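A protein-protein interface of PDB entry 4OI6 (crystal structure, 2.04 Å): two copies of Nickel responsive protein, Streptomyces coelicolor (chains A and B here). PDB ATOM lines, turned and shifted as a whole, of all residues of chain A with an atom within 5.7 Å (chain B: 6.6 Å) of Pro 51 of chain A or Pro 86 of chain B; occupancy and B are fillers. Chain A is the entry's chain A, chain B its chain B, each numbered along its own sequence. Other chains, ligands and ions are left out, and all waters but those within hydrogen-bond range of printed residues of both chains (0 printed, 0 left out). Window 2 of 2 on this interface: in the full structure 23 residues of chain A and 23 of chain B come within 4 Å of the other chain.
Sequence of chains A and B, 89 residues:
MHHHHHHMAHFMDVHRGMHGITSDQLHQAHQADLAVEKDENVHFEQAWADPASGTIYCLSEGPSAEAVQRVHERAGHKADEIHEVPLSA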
ATOM      1  N   MET A  18      34.623 -12.485 -24.287  1.00  0.00           N
ATOM      2  CA  MET A  18      34.422 -13.122 -22.988  1.00  0.00           C
ATOM      3  C   MET A  18      32.954 -13.495 -22.772  1.00  0.00           C
ATOM      4  O   MET A  18      32.419 -13.300 -21.670  1.00  0.00           O
ATOM      5  CB  MET A  18      34.865 -12.196 -21.844  1.00  0.00           C
ATOM      6  CG  MET A  18      36.320 -11.755 -21.894  1.00  0.00           C
ATOM      7  SD  MET A  18      37.493 -13.234 -22.320  1.00  0.00           S
ATOM      8  CE  MET A  18      37.209 -14.305 -20.709  1.00  0.00           C
ATOM      9  N   HIS A  19      32.294 -14.025 -23.799  1.00  0.00           N
ATOM     10  CA  HIS A  19      30.860 -14.320 -23.671  1.00  0.00           C
ATOM     11  C   HIS A  19      30.597 -15.305 -22.528  1.00  0.00           C
ATOM     12  O   HIS A  19      31.356 -16.245 -22.331  1.00  0.00           O
ATOM     13  CB  HIS A  19      30.301 -14.866 -24.991  1.00  0.00           C
ATOM     14  CG  HIS A  19      31.052 -16.044 -25.514  1.00  0.00           C
ATOM     15  ND1 HIS A  19      30.694 -17.346 -25.219  1.00  0.00           N
ATOM     16  CD2 HIS A  19      32.157 -16.127 -26.296  1.00  0.00           C
ATOM     17  CE1 HIS A  19      31.539 -18.175 -25.806  1.00  0.00           C
ATOM     18  NE2 HIS A  19      32.429 -17.466 -26.473  1.00  0.00           N
ATOM     19  N   GLY A  20      29.542 -15.066 -21.753  1.00  0.00           N
ATOM     20  CA  GLY A  20      29.160 -15.988 -20.691  1.00  0.00           C
ATOM     21  C   GLY A  20      30.050 -16.005 -19.454  1.00  0.00           C
ATOM     22  O   GLY A  20      29.825 -16.815 -18.555  1.00  0.00           O
ATOM     23  N   ILE A  21      31.046 -15.112 -19.402  1.00  0.00           N
ATOM     24  CA  ILE A  21      31.946 -15.005 -18.247  1.00  0.00           C
ATOM     25  C   ILE A  21      31.159 -14.869 -16.938  1.00  0.00           C
ATOM     26  O   ILE A  21      30.157 -14.149 -16.877  1.00  0.00           O
ATOM     27  CB  ILE A  21      32.965 -13.821 -18.427  1.00  0.00           C
ATOM     28  CG1 ILE A  21      34.067 -13.846 -17.369  1.00  0.00           C
ATOM     29  CG2 ILE A  21      32.272 -12.448 -18.423  1.00  0.00           C
ATOM     30  CD1 ILE A  21      35.078 -12.725 -17.564  1.00  0.00           C
ATOM     31  N   ALA A  49      32.216  -6.120 -16.407  1.00  0.00           N
ATOM     32  CA  ALA A  49      32.043  -7.077 -17.505  1.00  0.00           C
ATOM     33  C   ALA A  49      30.589  -7.240 -17.910  1.00  0.00           C
ATOM     34  O   ALA A  49      29.687  -7.230 -17.066  1.00  0.00           O
ATOM     35  CB  ALA A  49      32.659  -8.444 -17.170  1.00  0.00           C
ATOM     36  N   ASP A  50      30.388  -7.398 -19.216  1.00  0.00           N
ATOM     37  CA  ASP A  50      29.102  -7.677 -19.817  1.00  0.00           C
ATOM     38  C   ASP A  50      29.180  -9.085 -20.363  1.00  0.00           C
ATOM     39  O   ASP A  50      29.802  -9.307 -21.406  1.00  0.00           O
ATOM     40  CB  ASP A  50      28.860  -6.723 -20.979  1.00  0.00           C
ATOM     41  CG  ASP A  50      27.577  -7.031 -21.728  1.00  0.00           C
ATOM     42  OD1 ASP A  50      26.698  -7.711 -21.159  1.00  0.00           O
ATOM     43  OD2 ASP A  50      27.442  -6.581 -22.885  1.00  0.00           O
ATOM     44  N   PRO A  51      28.547 -10.045 -19.668  1.00  0.00           N
ATOM     45  CA  PRO A  51      28.617 -11.444 -20.116  1.00  0.00           C
ATOM     46  C   PRO A  51      27.779 -11.675 -21.378  1.00  0.00           C
ATOM     47  O   PRO A  51      28.002 -12.669 -22.070  1.00  0.00           O
ATOM     48  CB  PRO A  51      28.030 -12.238 -18.934  1.00  0.00           C
ATOM     49  CG  PRO A  51      27.860 -11.230 -17.791  1.00  0.00           C
ATOM     50  CD  PRO A  51      27.730  -9.882 -18.452  1.00  0.00           C
ATOM     51  N   ALA A  52      26.837 -10.775 -21.673  1.00  0.00           N
ATOM     52  CA  ALA A  52      25.996 -10.937 -22.859  1.00  0.00           C
ATOM     53  C   ALA A  52      26.804 -10.697 -24.135  1.00  0.00           C
ATOM     54  O   ALA A  52      26.848 -11.550 -25.025  1.00  0.00           O
ATOM     55  CB  ALA A  52      24.770 -10.020 -22.806  1.00  0.00           C
ATOM     56  N   SER A  53      27.432  -9.532 -24.235  1.00  0.00           N
ATOM     57  CA  SER A  53      28.257  -9.253 -25.409  1.00  0.00           C
ATOM     58  C   SER A  53      29.632  -9.880 -25.220  1.00  0.00           C
ATOM     59  O   SER A  53      30.336 -10.191 -26.189  1.00  0.00           O
ATOM     60  CB  SER A  53      28.353  -7.743 -25.680  1.00  0.00           C
ATOM     61  OG  SER A  53      28.929  -7.046 -24.581  1.00  0.00           O
ATOM     62  N   GLY A  54      30.008 -10.094 -23.965  1.00  0.00           N
ATOM     63  CA  GLY A  54      31.300 -10.671 -23.668  1.00  0.00           C
ATOM     64  C   GLY A  54      32.371  -9.593 -23.619  1.00  0.00           C
ATOM     65  O   GLY A  54      33.530  -9.853 -23.963  1.00  0.00           O
ATOM     66  N   THR A  55      31.990  -8.388 -23.185  1.00  0.00           N
ATOM     67  CA  THR A  55      32.938  -7.272 -23.180  1.00  0.00           C
ATOM     68  C   THR A  55      33.390  -6.914 -21.765  1.00  0.00           C
ATOM     69  O   THR A  55      32.569  -6.734 -20.873  1.00  0.00           O
ATOM     70  CB  THR A  55      32.339  -6.018 -23.841  1.00  0.00           C
ATOM     71  OG1 THR A  55      31.770  -6.371 -25.109  1.00  0.00           O
ATOM     72  CG2 THR A  55      33.424  -4.936 -24.059  1.00  0.00           C
ATOM     73  N   HIS B  10      23.678  -1.502 -14.015  1.00  0.00           N
ATOM     74  CA  HIS B  10      24.765  -0.604 -14.435  1.00  0.00           C
ATOM     75  C   HIS B  10      25.083  -0.758 -15.925  1.00  0.00           C
ATOM     76  O   HIS B  10      24.922  -1.846 -16.499  1.00  0.00           O
ATOM     77  CB  HIS B  10      26.051  -0.849 -13.638  1.00  0.00           C
ATOM     78  CG  HIS B  10      26.025  -0.317 -12.243  1.00  0.00           C
ATOM     79  ND1 HIS B  10      25.372  -0.960 -11.208  1.00  0.00           N
ATOM     80  CD2 HIS B  10      26.604   0.782 -11.694  1.00  0.00           C
ATOM     81  CE1 HIS B  10      25.537  -0.272 -10.092  1.00  0.00           C
ATOM     82  NE2 HIS B  10      26.282   0.786 -10.357  1.00  0.00           N
ATOM     83  N   HIS B  83      26.431  -1.135 -23.203  1.00  0.00           N
ATOM     84  CA  HIS B  83      26.338  -2.504 -22.698  1.00  0.00           C
ATOM     85  C   HIS B  83      25.988  -2.486 -21.210  1.00  0.00           C
ATOM     86  O   HIS B  83      26.549  -1.690 -20.445  1.00  0.00           O
ATOM     87  CB  HIS B  83      27.665  -3.249 -22.910  1.00  0.00           C
ATOM     88  CG  HIS B  83      28.128  -3.282 -24.337  1.00  0.00           C
ATOM     89  ND1 HIS B  83      27.540  -4.084 -25.292  1.00  0.00           N
ATOM     90  CD2 HIS B  83      29.117  -2.607 -24.970  1.00  0.00           C
ATOM     91  CE1 HIS B  83      28.150  -3.905 -26.451  1.00  0.00           C
ATOM     92  NE2 HIS B  83      29.112  -3.011 -26.283  1.00  0.00           N
ATOM     93  N   GLU B  84      25.053  -3.338 -20.792  1.00  0.00           N
ATOM     94  CA  GLU B  84      24.826  -3.522 -19.361  1.00  0.00           C
ATOM     95  C   GLU B  84      26.046  -4.238 -18.790  1.00  0.00           C
ATOM     96  O   GLU B  84      26.563  -5.163 -19.420  1.00  0.00           O
ATOM     97  CB  GLU B  84      23.579  -4.359 -19.098  1.00  0.00           C
ATOM     98  CG  GLU B  84      23.245  -4.458 -17.606  1.00  0.00           C
ATOM     99  CD  GLU B  84      22.032  -5.323 -17.310  1.00  0.00           C
ATOM    100  OE1 GLU B  84      21.183  -5.514 -18.214  1.00  0.00           O
ATOM    101  OE2 GLU B  84      21.937  -5.808 -16.163  1.00  0.00           O
ATOM    102  N   VAL B  85      26.519  -3.810 -17.619  1.00  0.00           N
ATOM    103  CA  VAL B  85      27.658  -4.473 -16.970  1.00  0.00           C
ATOM    104  C   VAL B  85      27.274  -4.973 -15.571  1.00  0.00           C
ATOM    105  O   VAL B  85      27.572  -4.332 -14.568  1.00  0.00           O
ATOM    106  CB  VAL B  85      28.952  -3.585 -16.943  1.00  0.00           C
ATOM    107  CG1 VAL B  85      29.541  -3.436 -18.345  1.00  0.00           C
ATOM    108  CG2 VAL B  85      28.675  -2.199 -16.362  1.00  0.00           C
ATOM    109  N   PRO B  86      26.605  -6.139 -15.506  1.00  0.00           N
ATOM    110  CA  PRO B  86      26.123  -6.636 -14.209  1.00  0.00           C
ATOM    111  C   PRO B  86      27.258  -7.218 -13.358  1.00  0.00           C
ATOM    112  O   PRO B  86      27.047  -7.528 -12.178  1.00  0.00           O
ATOM    113  CB  PRO B  86      25.123  -7.726 -14.607  1.00  0.00           C
ATOM    114  CG  PRO B  86      25.665  -8.252 -15.926  1.00  0.00           C
ATOM    115  CD  PRO B  86      26.293  -7.063 -16.616  1.00  0.00           C
ATOM    116  N   LEU B  87      28.448  -7.357 -13.944  1.00  0.00           N
ATOM    117  CA  LEU B  87      29.585  -7.890 -13.209  1.00  0.00           C
ATOM    118  C   LEU B  87      30.632  -6.804 -13.015  1.00  0.00           C
ATOM    119  O   LEU B  87      30.949  -6.057 -13.950  1.00  0.00           O
ATOM    120  CB  LEU B  87      30.218  -9.058 -13.960  1.00  0.00           C
ATOM    121  CG  LEU B  87      29.312 -10.230 -14.332  1.00  0.00           C
ATOM    122  CD1 LEU B  87      30.168 -11.345 -14.917  1.00  0.00           C
ATOM    123  CD2 LEU B  87      28.542 -10.722 -13.124  1.00  0.00           C
ATOM    124  N   SER B  88      31.171  -6.720 -11.803  1.00  0.00           N
ATOM    125  CA  SER B  88      32.232  -5.767 -11.521  1.00  0.00           C
ATOM    126  C   SER B  88      33.173  -6.336 -10.476  1.00  0.00           C
ATOM    127  O   SER B  88      32.780  -7.215  -9.696  1.00  0.00           O
ATOM    128  CB  SER B  88      31.643  -4.447 -11.037  1.00  0.00           C
ATOM    129  OG  SER B  88      30.848  -4.651  -9.885  1.00  0.00           O
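The backbone NH (N) of Ala 49 of chain A sits at hydrogen-bond distance from the backbone carbonyl oxygen (O) of Leu 87 of chain B.
ND1 of His 83 of chain B lies close to OD2 of Asp 50 of chain A (3.5 Å).
ND1 of His 83 of chain B lies within hydrogen-bond range of OG of Ser 53 of chain A (3.3 Å).
OD1 of Asp 50 of chain A sits close to O of Glu 84 of chain B, at 3.1 Å.
N of Gly 20 of chain A lies within hydrogen-bond range of O of Pro 51 of chain A (2.9 Å).
The side-chain carboxylate (OD1) of Asp 50 of chain A sits at hydrogen-bond distance from the backbone NH (N) of Ala 52 of chain A, 3.1 Å away.
The backbone NH (N) of Ser 53 of chain A sits close to the side-chain carboxylate (OD2) of Asp 50 of chain A (3.2 Å).
N of Asp 50 of chain A is in hydrogen-bond range of O of Thr 55 of chain A (2.8 Å).
OG of Ser 53 of chain A sits at hydrogen-bond distance from OG1 of Thr 55 of chain A, at 3.0 Å.
The backbone carbonyl oxygen (O) of His 10 of chain B is in hydrogen-bond range of the backbone NH (N) of Val 85 of chain B, 2.8 Å away.
Among the printed residues, merely in contact across the chains: Ile 21 of chain A with Leu 87 of chain B (3.4 Å), Ala 49 of chain A with Val 85 of chain B (3.4 Å), Ala 49 of chain A with Pro 86 of chain B (3.4 Å), Pro 51 of chain A with Pro 86 of chain B (3.6 Å) and Pro 51 of chain A with Leu 87 of chain B (3.7 Å).
Printed residues of chain A within 4 Å of His 83 of chain B: Asp 50 (3.3 Å) and Ser 53 (3.3 Å).
Printed residues of chain A within 4 Å of Leu 87 of chain B: Ile 21, Ala 49 and Pro 51.
Of the printed residues of chain B, Ala 49 of chain A touches Val 85 (3.4 Å), Pro 86 (3.4 Å) and Leu 87 (2.8 Å).
Printed residues of chain B within 4 Å of Asp 50 of chain A: His 83 and Glu 84.
Met 18 of chain A touches none of the printed residues of chain B.
Thr 55 of chain A touches none of the printed residues of chain B.
The nearest printed residue of chain B that does not touch Ile 21 of chain A is Pro 86 of chain B (7.5 Å).
Of the 11 printed residues of chain A, 5 touch a printed residue of chain B.
Of the 7 printed residues of chain B, 5 touch a printed residue of chain A.
Hydrophobic or aromatic side chains of chain B within 4 Å of the printed part of chain A: His 83, Val 85, Pro 86 and Leu 87.
Among the printed residues, 9 pairs touch across the chains.
No position is printed for both chains.
Of the 9 pairs that touch across the chains among the printed residues, none has its exchanged pair printed and touching as well.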
